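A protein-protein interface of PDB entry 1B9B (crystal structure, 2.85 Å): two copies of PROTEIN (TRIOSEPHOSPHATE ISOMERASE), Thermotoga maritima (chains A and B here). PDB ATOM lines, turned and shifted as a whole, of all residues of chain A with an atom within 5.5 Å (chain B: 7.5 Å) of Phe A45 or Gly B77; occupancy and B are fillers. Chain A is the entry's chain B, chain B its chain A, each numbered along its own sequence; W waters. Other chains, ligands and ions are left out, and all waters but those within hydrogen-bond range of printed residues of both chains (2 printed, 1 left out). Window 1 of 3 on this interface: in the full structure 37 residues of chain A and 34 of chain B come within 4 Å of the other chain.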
ATOM      1  N   LYS A  12     -27.318  29.211  18.224  1.00  0.00           N
ATOM      2  CA  LYS A  12     -27.575  28.879  16.826  1.00  0.00           C
ATOM      3  C   LYS A  12     -26.327  28.184  16.298  1.00  0.00           C
ATOM      4  O   LYS A  12     -25.627  27.527  17.067  1.00  0.00           O
ATOM      5  CB  LYS A  12     -27.897  30.128  16.001  1.00  0.00           C
ATOM      6  CG  LYS A  12     -29.123  30.866  16.508  1.00  0.00           C
ATOM      7  CD  LYS A  12     -29.702  31.812  15.472  1.00  0.00           C
ATOM      8  CE  LYS A  12     -30.965  32.452  16.014  1.00  0.00           C
ATOM      9  NZ  LYS A  12     -31.561  33.424  15.069  1.00  0.00           N
ATOM     10  N   PRO A  43     -25.969  25.424  23.199  1.00  0.00           N
ATOM     11  CA  PRO A  43     -24.898  25.223  22.217  1.00  0.00           C
ATOM     12  C   PRO A  43     -25.281  24.181  21.164  1.00  0.00           C
ATOM     13  O   PRO A  43     -26.254  23.450  21.342  1.00  0.00           O
ATOM     14  CB  PRO A  43     -23.727  24.767  23.083  1.00  0.00           C
ATOM     15  CG  PRO A  43     -24.407  24.002  24.176  1.00  0.00           C
ATOM     16  CD  PRO A  43     -25.594  24.865  24.513  1.00  0.00           C
ATOM     17  N   PRO A  44     -24.532  24.115  20.044  1.00  0.00           N
ATOM     18  CA  PRO A  44     -24.803  23.148  18.971  1.00  0.00           C
ATOM     19  C   PRO A  44     -24.551  21.732  19.478  1.00  0.00           C
ATOM     20  O   PRO A  44     -23.732  21.533  20.372  1.00  0.00           O
ATOM     21  CB  PRO A  44     -23.805  23.545  17.890  1.00  0.00           C
ATOM     22  CG  PRO A  44     -23.636  25.012  18.107  1.00  0.00           C
ATOM     23  CD  PRO A  44     -23.538  25.110  19.606  1.00  0.00           C
ATOM     24  N   PHE A  45     -25.251  20.753  18.916  1.00  0.00           N
ATOM     25  CA  PHE A  45     -25.086  19.357  19.335  1.00  0.00           C
ATOM     26  C   PHE A  45     -23.624  18.963  19.534  1.00  0.00           C
ATOM     27  O   PHE A  45     -23.250  18.426  20.580  1.00  0.00           O
ATOM     28  CB  PHE A  45     -25.693  18.409  18.300  1.00  0.00           C
ATOM     29  CG  PHE A  45     -27.164  18.554  18.129  1.00  0.00           C
ATOM     30  CD1 PHE A  45     -28.025  18.360  19.209  1.00  0.00           C
ATOM     31  CD2 PHE A  45     -27.698  18.852  16.884  1.00  0.00           C
ATOM     32  CE1 PHE A  45     -29.401  18.457  19.049  1.00  0.00           C
ATOM     33  CE2 PHE A  45     -29.070  18.952  16.712  1.00  0.00           C
ATOM     34  CZ  PHE A  45     -29.925  18.753  17.797  1.00  0.00           C
ATOM     35  N   THR A  46     -22.810  19.217  18.513  1.00  0.00           N
ATOM     36  CA  THR A  46     -21.393  18.884  18.545  1.00  0.00           C
ATOM     37  C   THR A  46     -20.748  19.225  19.878  1.00  0.00           C
ATOM     38  O   THR A  46     -19.969  18.435  20.413  1.00  0.00           O
ATOM     39  CB  THR A  46     -20.624  19.621  17.431  1.00  0.00           C
ATOM     40  OG1 THR A  46     -20.751  21.038  17.611  1.00  0.00           O
ATOM     41  CG2 THR A  46     -21.160  19.225  16.064  1.00  0.00           C
ATOM     42  N   ALA A  47     -21.095  20.390  20.422  1.00  0.00           N
ATOM     43  CA  ALA A  47     -20.517  20.858  21.679  1.00  0.00           C
ATOM     44  C   ALA A  47     -21.390  20.807  22.932  1.00  0.00           C
ATOM     45  O   ALA A  47     -21.307  21.701  23.765  1.00  0.00           O
ATOM     46  CB  ALA A  47     -20.009  22.271  21.489  1.00  0.00           C
ATOM     47  N   LEU A  48     -22.211  19.779  23.093  1.00  0.00           N
ATOM     48  CA  LEU A  48     -23.051  19.711  24.284  1.00  0.00           C
ATOM     49  C   LEU A  48     -22.379  18.970  25.415  1.00  0.00           C
ATOM     50  O   LEU A  48     -22.414  19.409  26.554  1.00  0.00           O
ATOM     51  CB  LEU A  48     -24.389  19.032  23.985  1.00  0.00           C
ATOM     52  CG  LEU A  48     -25.390  19.769  23.098  1.00  0.00           C
ATOM     53  CD1 LEU A  48     -26.625  18.903  22.931  1.00  0.00           C
ATOM     54  CD2 LEU A  48     -25.757  21.101  23.713  1.00  0.00           C
ATOM     55  N   SER A  49     -21.784  17.831  25.095  1.00  0.00           N
ATOM     56  CA  SER A  49     -21.106  17.004  26.089  1.00  0.00           C
ATOM     57  C   SER A  49     -20.026  17.764  26.842  1.00  0.00           C
ATOM     58  O   SER A  49     -19.869  17.607  28.051  1.00  0.00           O
ATOM     59  CB  SER A  49     -20.475  15.780  25.418  1.00  0.00           C
ATOM     60  OG  SER A  49     -19.615  15.097  26.315  1.00  0.00           O
ATOM     61  N   ALA A  64     -30.845  22.380  24.236  1.00  0.00           N
ATOM     62  CA  ALA A  64     -30.562  22.037  22.839  1.00  0.00           C
ATOM     63  C   ALA A  64     -31.390  22.901  21.888  1.00  0.00           C
ATOM     64  O   ALA A  64     -32.417  23.455  22.271  1.00  0.00           O
ATOM     65  CB  ALA A  64     -30.850  20.568  22.595  1.00  0.00           C
ATOM     66  N   GLN A  65     -30.942  23.004  20.644  1.00  0.00           N
ATOM     67  CA  GLN A  65     -31.621  23.822  19.642  1.00  0.00           C
ATOM     68  C   GLN A  65     -32.627  23.077  18.772  1.00  0.00           C
ATOM     69  O   GLN A  65     -33.259  23.676  17.894  1.00  0.00           O
ATOM     70  CB  GLN A  65     -30.588  24.481  18.734  1.00  0.00           C
ATOM     71  CG  GLN A  65     -29.714  25.502  19.427  1.00  0.00           C
ATOM     72  CD  GLN A  65     -28.524  25.901  18.584  1.00  0.00           C
ATOM     73  OE1 GLN A  65     -28.639  26.071  17.366  1.00  0.00           O
ATOM     74  NE2 GLN A  65     -27.368  26.060  19.229  1.00  0.00           N
ATOM     75  N   ASN A  66     -32.774  21.776  19.004  1.00  0.00           N
ATOM     76  CA  ASN A  66     -33.709  20.981  18.221  1.00  0.00           C
ATOM     77  C   ASN A  66     -33.648  19.528  18.663  1.00  0.00           C
ATOM     78  O   ASN A  66     -32.696  19.124  19.320  1.00  0.00           O
ATOM     79  CB  ASN A  66     -33.369  21.118  16.728  1.00  0.00           C
ATOM     80  CG  ASN A  66     -34.331  20.364  15.822  1.00  0.00           C
ATOM     81  OD1 ASN A  66     -35.553  20.424  15.986  1.00  0.00           O
ATOM     82  ND2 ASN A  66     -33.776  19.661  14.843  1.00  0.00           N
ATOM     83  N   VAL A  67     -34.680  18.757  18.316  1.00  0.00           N
ATOM     84  CA  VAL A  67     -34.764  17.333  18.657  1.00  0.00           C
ATOM     85  C   VAL A  67     -35.701  16.645  17.680  1.00  0.00           C
ATOM     86  O   VAL A  67     -36.514  17.300  17.030  1.00  0.00           O
ATOM     87  CB  VAL A  67     -35.375  17.103  20.062  1.00  0.00           C
ATOM     88  CG1 VAL A  67     -35.232  15.649  20.472  1.00  0.00           C
ATOM     89  CG2 VAL A  67     -34.695  17.964  21.064  1.00  0.00           C
ATOM     90  N   ILE A  79     -31.178  13.798  16.106  1.00  0.00           N
ATOM     91  CA  ILE A  79     -30.860  13.596  17.519  1.00  0.00           C
ATOM     92  C   ILE A  79     -32.123  13.190  18.271  1.00  0.00           C
ATOM     93  O   ILE A  79     -33.186  13.757  18.046  1.00  0.00           O
ATOM     94  CB  ILE A  79     -30.296  14.898  18.142  1.00  0.00           C
ATOM     95  CG1 ILE A  79     -29.057  15.331  17.365  1.00  0.00           C
ATOM     96  CG2 ILE A  79     -29.954  14.701  19.618  1.00  0.00           C
ATOM     97  CD1 ILE A  79     -27.992  14.287  17.281  1.00  0.00           C
ATOM     98  N   LEU A  84     -30.151  13.491  24.307  1.00  0.00           N
ATOM     99  CA  LEU A  84     -30.080  14.773  25.003  1.00  0.00           C
ATOM    100  C   LEU A  84     -30.216  14.591  26.507  1.00  0.00           C
ATOM    101  O   LEU A  84     -29.549  15.264  27.298  1.00  0.00           O
ATOM    102  CB  LEU A  84     -31.184  15.702  24.507  1.00  0.00           C
ATOM    103  CG  LEU A  84     -30.963  16.257  23.101  1.00  0.00           C
ATOM    104  CD1 LEU A  84     -32.110  17.155  22.698  1.00  0.00           C
ATOM    105  CD2 LEU A  84     -29.661  17.032  23.064  1.00  0.00           C
ATOM    106  N   ARG A  99     -36.238  26.913  11.508  1.00  0.00           N
ATOM    107  CA  ARG A  99     -36.596  25.541  11.192  1.00  0.00           C
ATOM    108  C   ARG A  99     -37.936  25.498  10.435  1.00  0.00           C
ATOM    109  O   ARG A  99     -38.082  24.770   9.456  1.00  0.00           O
ATOM    110  CB  ARG A  99     -36.642  24.715  12.477  1.00  0.00           C
ATOM    111  CG  ARG A  99     -35.317  24.741  13.251  1.00  0.00           C
ATOM    112  CD  ARG A  99     -34.964  23.373  13.836  1.00  0.00           C
ATOM    113  NE  ARG A  99     -34.942  22.329  12.808  1.00  0.00           N
ATOM    114  CZ  ARG A  99     -33.962  22.137  11.926  1.00  0.00           C
ATOM    115  NH1 ARG A  99     -32.886  22.912  11.932  1.00  0.00           N
ATOM    116  NH2 ARG A  99     -34.073  21.178  11.018  1.00  0.00           N
ATOM    117  N   ILE B  17     -23.720   8.601  24.297  1.00  0.00           N
ATOM    118  CA  ILE B  17     -22.281   8.790  24.466  1.00  0.00           C
ATOM    119  C   ILE B  17     -21.643   7.676  25.294  1.00  0.00           C
ATOM    120  O   ILE B  17     -20.506   7.276  25.052  1.00  0.00           O
ATOM    121  CB  ILE B  17     -21.978  10.150  25.102  1.00  0.00           C
ATOM    122  CG1 ILE B  17     -22.394  11.257  24.130  1.00  0.00           C
ATOM    123  CG2 ILE B  17     -20.498  10.253  25.453  1.00  0.00           C
ATOM    124  CD1 ILE B  17     -22.113  12.657  24.628  1.00  0.00           C
ATOM    125  N   PRO B  44     -23.825   9.860  15.971  1.00  0.00           N
ATOM    126  CA  PRO B  44     -24.601  11.104  15.950  1.00  0.00           C
ATOM    127  C   PRO B  44     -23.803  12.290  16.496  1.00  0.00           C
ATOM    128  O   PRO B  44     -22.844  12.107  17.238  1.00  0.00           O
ATOM    129  CB  PRO B  44     -25.827  10.757  16.792  1.00  0.00           C
ATOM    130  CG  PRO B  44     -25.317   9.694  17.726  1.00  0.00           C
ATOM    131  CD  PRO B  44     -24.462   8.849  16.833  1.00  0.00           C
ATOM    132  N   PHE B  45     -24.196  13.501  16.126  1.00  0.00           N
ATOM    133  CA  PHE B  45     -23.484  14.695  16.567  1.00  0.00           C
ATOM    134  C   PHE B  45     -23.112  14.717  18.037  1.00  0.00           C
ATOM    135  O   PHE B  45     -21.977  15.035  18.392  1.00  0.00           O
ATOM    136  CB  PHE B  45     -24.299  15.940  16.252  1.00  0.00           C
ATOM    137  CG  PHE B  45     -24.576  16.113  14.805  1.00  0.00           C
ATOM    138  CD1 PHE B  45     -23.536  16.174  13.894  1.00  0.00           C
ATOM    139  CD2 PHE B  45     -25.875  16.220  14.347  1.00  0.00           C
ATOM    140  CE1 PHE B  45     -23.786  16.337  12.542  1.00  0.00           C
ATOM    141  CE2 PHE B  45     -26.134  16.385  13.001  1.00  0.00           C
ATOM    142  CZ  PHE B  45     -25.089  16.444  12.097  1.00  0.00           C
ATOM    143  N   THR B  46     -24.066  14.389  18.898  1.00  0.00           N
ATOM    144  CA  THR B  46     -23.809  14.408  20.332  1.00  0.00           C
ATOM    145  C   THR B  46     -22.528  13.681  20.751  1.00  0.00           C
ATOM    146  O   THR B  46     -21.741  14.216  21.530  1.00  0.00           O
ATOM    147  CB  THR B  46     -25.011  13.830  21.128  1.00  0.00           C
ATOM    148  OG1 THR B  46     -25.394  12.563  20.584  1.00  0.00           O
ATOM    149  CG2 THR B  46     -26.187  14.779  21.063  1.00  0.00           C
ATOM    150  N   ALA B  47     -22.308  12.483  20.212  1.00  0.00           N
ATOM    151  CA  ALA B  47     -21.138  11.674  20.559  1.00  0.00           C
ATOM    152  C   ALA B  47     -19.886  11.858  19.705  1.00  0.00           C
ATOM    153  O   ALA B  47     -18.917  11.124  19.879  1.00  0.00           O
ATOM    154  CB  ALA B  47     -21.529  10.198  20.555  1.00  0.00           C
ATOM    155  N   LEU B  48     -19.884  12.828  18.799  1.00  0.00           N
ATOM    156  CA  LEU B  48     -18.720  13.012  17.945  1.00  0.00           C
ATOM    157  C   LEU B  48     -17.401  13.276  18.658  1.00  0.00           C
ATOM    158  O   LEU B  48     -16.444  12.537  18.463  1.00  0.00           O
ATOM    159  CB  LEU B  48     -18.963  14.116  16.917  1.00  0.00           C
ATOM    160  CG  LEU B  48     -19.925  13.756  15.788  1.00  0.00           C
ATOM    161  CD1 LEU B  48     -19.849  14.824  14.703  1.00  0.00           C
ATOM    162  CD2 LEU B  48     -19.571  12.381  15.227  1.00  0.00           C
ATOM    163  N   SER B  49     -17.334  14.314  19.482  1.00  0.00           N
ATOM    164  CA  SER B  49     -16.075  14.605  20.151  1.00  0.00           C
ATOM    165  C   SER B  49     -15.586  13.471  21.052  1.00  0.00           C
ATOM    166  O   SER B  49     -14.399  13.160  21.067  1.00  0.00           O
ATOM    167  CB  SER B  49     -16.180  15.898  20.954  1.00  0.00           C
ATOM    168  OG  SER B  49     -17.080  15.746  22.025  1.00  0.00           O
ATOM    169  N   ALA B  74     -27.423  32.115  11.465  1.00  0.00           N
ATOM    170  CA  ALA B  74     -28.655  31.861  12.192  1.00  0.00           C
ATOM    171  C   ALA B  74     -29.445  30.742  11.529  1.00  0.00           C
ATOM    172  O   ALA B  74     -30.327  30.977  10.692  1.00  0.00           O
ATOM    173  CB  ALA B  74     -29.489  33.118  12.264  1.00  0.00           C
ATOM    174  N   PHE B  75     -29.092  29.519  11.908  1.00  0.00           N
ATOM    175  CA  PHE B  75     -29.736  28.312  11.422  1.00  0.00           C
ATOM    176  C   PHE B  75     -29.809  27.406  12.637  1.00  0.00           C
ATOM    177  O   PHE B  75     -29.040  26.457  12.783  1.00  0.00           O
ATOM    178  CB  PHE B  75     -28.910  27.660  10.316  1.00  0.00           C
ATOM    179  CG  PHE B  75     -28.613  28.578   9.163  1.00  0.00           C
ATOM    180  CD1 PHE B  75     -29.489  28.671   8.089  1.00  0.00           C
ATOM    181  CD2 PHE B  75     -27.456  29.359   9.154  1.00  0.00           C
ATOM    182  CE1 PHE B  75     -29.214  29.526   7.024  1.00  0.00           C
ATOM    183  CE2 PHE B  75     -27.175  30.214   8.095  1.00  0.00           C
ATOM    184  CZ  PHE B  75     -28.054  30.297   7.030  1.00  0.00           C
ATOM    185  N   THR B  76     -30.735  27.746  13.524  1.00  0.00           N
ATOM    186  CA  THR B  76     -30.950  27.017  14.756  1.00  0.00           C
ATOM    187  C   THR B  76     -31.057  25.520  14.515  1.00  0.00           C
ATOM    188  O   THR B  76     -31.794  25.080  13.638  1.00  0.00           O
ATOM    189  CB  THR B  76     -32.239  27.502  15.431  1.00  0.00           C
ATOM    190  OG1 THR B  76     -32.191  28.927  15.559  1.00  0.00           O
ATOM    191  CG2 THR B  76     -32.401  26.876  16.810  1.00  0.00           C
ATOM    192  N   GLY B  77     -30.311  24.741  15.293  1.00  0.00           N
ATOM    193  CA  GLY B  77     -30.363  23.297  15.164  1.00  0.00           C
ATOM    194  C   GLY B  77     -29.366  22.626  14.232  1.00  0.00           C
ATOM    195  O   GLY B  77     -29.111  21.429  14.375  1.00  0.00           O
ATOM    196  N   GLU B  78     -28.802  23.383  13.293  1.00  0.00           N
ATOM    197  CA  GLU B  78     -27.848  22.852  12.321  1.00  0.00           C
ATOM    198  C   GLU B  78     -26.388  22.851  12.774  1.00  0.00           C
ATOM    199  O   GLU B  78     -26.000  23.614  13.661  1.00  0.00           O
ATOM    200  CB  GLU B  78     -27.962  23.642  11.023  1.00  0.00           C
ATOM    201  CG  GLU B  78     -29.337  23.595  10.399  1.00  0.00           C
ATOM    202  CD  GLU B  78     -29.688  22.228   9.838  1.00  0.00           C
ATOM    203  OE1 GLU B  78     -29.045  21.810   8.851  1.00  0.00           O
ATOM    204  OE2 GLU B  78     -30.607  21.576  10.385  1.00  0.00           O
ATOM    205  N   ILE B  79     -25.585  21.982  12.154  1.00  0.00           N
ATOM    206  CA  ILE B  79     -24.156  21.882  12.459  1.00  0.00           C
ATOM    207  C   ILE B  79     -23.347  22.318  11.241  1.00  0.00           C
ATOM    208  O   ILE B  79     -23.638  21.909  10.121  1.00  0.00           O
ATOM    209  CB  ILE B  79     -23.746  20.449  12.816  1.00  0.00           C
ATOM    210  CG1 ILE B  79     -24.561  19.950  14.007  1.00  0.00           C
ATOM    211  CG2 ILE B  79     -22.269  20.410  13.145  1.00  0.00           C
ATOM    212  CD1 ILE B  79     -24.416  20.783  15.264  1.00  0.00           C
ATOM    213  N   MET B  83     -17.500  22.954  12.684  1.00  0.00           N
ATOM    214  CA  MET B  83     -17.708  22.159  13.880  1.00  0.00           C
ATOM    215  C   MET B  83     -17.320  20.697  13.699  1.00  0.00           C
ATOM    216  O   MET B  83     -16.841  20.059  14.641  1.00  0.00           O
ATOM    217  CB  MET B  83     -19.165  22.269  14.320  1.00  0.00           C
ATOM    218  CG  MET B  83     -19.525  23.630  14.893  1.00  0.00           C
ATOM    219  SD  MET B  83     -21.300  23.862  15.110  1.00  0.00           S
ATOM    220  CE  MET B  83     -21.542  25.391  14.242  1.00  0.00           C
ATOM    221  N   ILE B  87     -13.419  18.567  15.041  1.00  0.00           N
ATOM    222  CA  ILE B  87     -13.481  17.310  15.779  1.00  0.00           C
ATOM    223  C   ILE B  87     -12.699  16.220  15.045  1.00  0.00           C
ATOM    224  O   ILE B  87     -12.480  15.132  15.576  1.00  0.00           O
ATOM    225  CB  ILE B  87     -14.946  16.851  15.999  1.00  0.00           C
ATOM    226  CG1 ILE B  87     -15.731  17.950  16.710  1.00  0.00           C
ATOM    227  CG2 ILE B  87     -14.987  15.600  16.862  1.00  0.00           C
ATOM    228  CD1 ILE B  87     -17.137  17.549  17.088  1.00  0.00           C
HETATM  229  O   HOH W   1     -19.087  17.862  23.292  1.00  0.00           O
HETATM  230  O   HOH W   2     -26.901  23.533  16.259  1.00  0.00           O
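O of Thr B76 lies within hydrogen-bond range of NH1 of Arg A99, 3.0 Å away.
The backbone NH (N) of Gly B77 is in hydrogen-bond range of the side-chain amide oxygen (OE1) of Gln A65, at 3.0 Å.
OE2 of Glu B78 is in salt-bridge range of NH1 of Arg A99 (3.1 Å).
The backbone carbonyl oxygen (O) of Lys A12 lies within hydrogen-bond range of the side-chain amide nitrogen (NE2) of Gln A65 (3.1 Å).
Among the printed residues, pairs that only touch across the chains: Thr A46 with Ile B79 (3.3 Å), Phe A45 with Gly B77 (3.4 Å), Lys A12 with Ala B74 (3.4 Å), Gln A65 with Thr B76 (3.5 Å), Phe A45 with Phe B45 (3.5 Å), Ser A49 with Ile B17 (3.6 Å), Phe A45 with Ile B79 (3.7 Å), Lys A12 with Thr B76 (3.8 Å), Pro A44 with Met B83 (3.8 Å), Thr A46 with Met B83 (3.8 Å), Pro A44 with Ile B79 (3.9 Å) and Thr A46 with Phe B45 (3.9 Å).
Phe A45 touches three residues of chain B.
Printed residues of chain B within 4 Å of Gln A65: Thr B76 (3.5 Å) and Gly B77 (3.0 Å).
Printed residues of chain A within 4 Å of Ala B74: Lys A12 (3.4 Å).
Gly B77 touches two residues of chain A.
Of the printed residues of chain A, Ile B79 touches Pro A44, Phe A45 and Thr A46.
The nearest residue of chain B that does not touch Phe A45 is Thr B46 (4.1 Å).
The nearest residue of chain A that does not touch Gly B77 is Asn A66 (4.03 Å).
The nearest printed residue of chain A that does not touch Glu B78 is Pro A44 (4.8 Å).
Hydrophobic or aromatic side chains of chain B that line the printed part of chain A: Ile B17, Phe B45, Ala B74, Ile B79 and Met B83.
Of the 15 printed residues of chain A, 7 touch a printed residue of chain B.
Printed residues of chain A that touch a printed residue of chain B: Lys A12, Pro A44, Phe A45, Thr A46, Ser A49, Gln A65 and Arg A99.
Hydrophobic or aromatic side chains of chain A within 4 Å of the printed part of chain B: Pro A44 and Phe A45.
Among the printed residues, 15 pairs touch across the chains.
Among the printed residues, Asp or Glu carboxylates within 4 Å of a Lys or Arg side-chain nitrogen of the other chain: Arg A99 with Glu B78 (3.1 Å).
Phe A45 touches its own counterpart, Phe B45.
Phe A45 touches Ile B79, but with the chains exchanged Ile A79 does not touch Phe B45 (4.04 Å).
Thr A46 touches Phe B45, but with the chains exchanged Phe A45 does not touch Thr B46 (4.1 Å).
Thr A46 touches Ile B79, but with the chains exchanged Ile A79 does not touch Thr B46 (4.04 Å).
Positions printed for both chains: 44, 45, 46, 47, 48, 49 and 79.
Of the 15 pairs that touch across the chains among the printed residues, 1 has its exchanged pair printed and touching as well.
Water W2 lies within hydrogen-bond range of O of Glu B78 (2.8 Å) and OE1 of Gln A65 (3.3 Å).
Water W1 lies within hydrogen-bond range of O of Thr A46 (3.1 Å), OG of Ser B49 (3.2 Å) and N of Ser A49 (3.2 Å).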
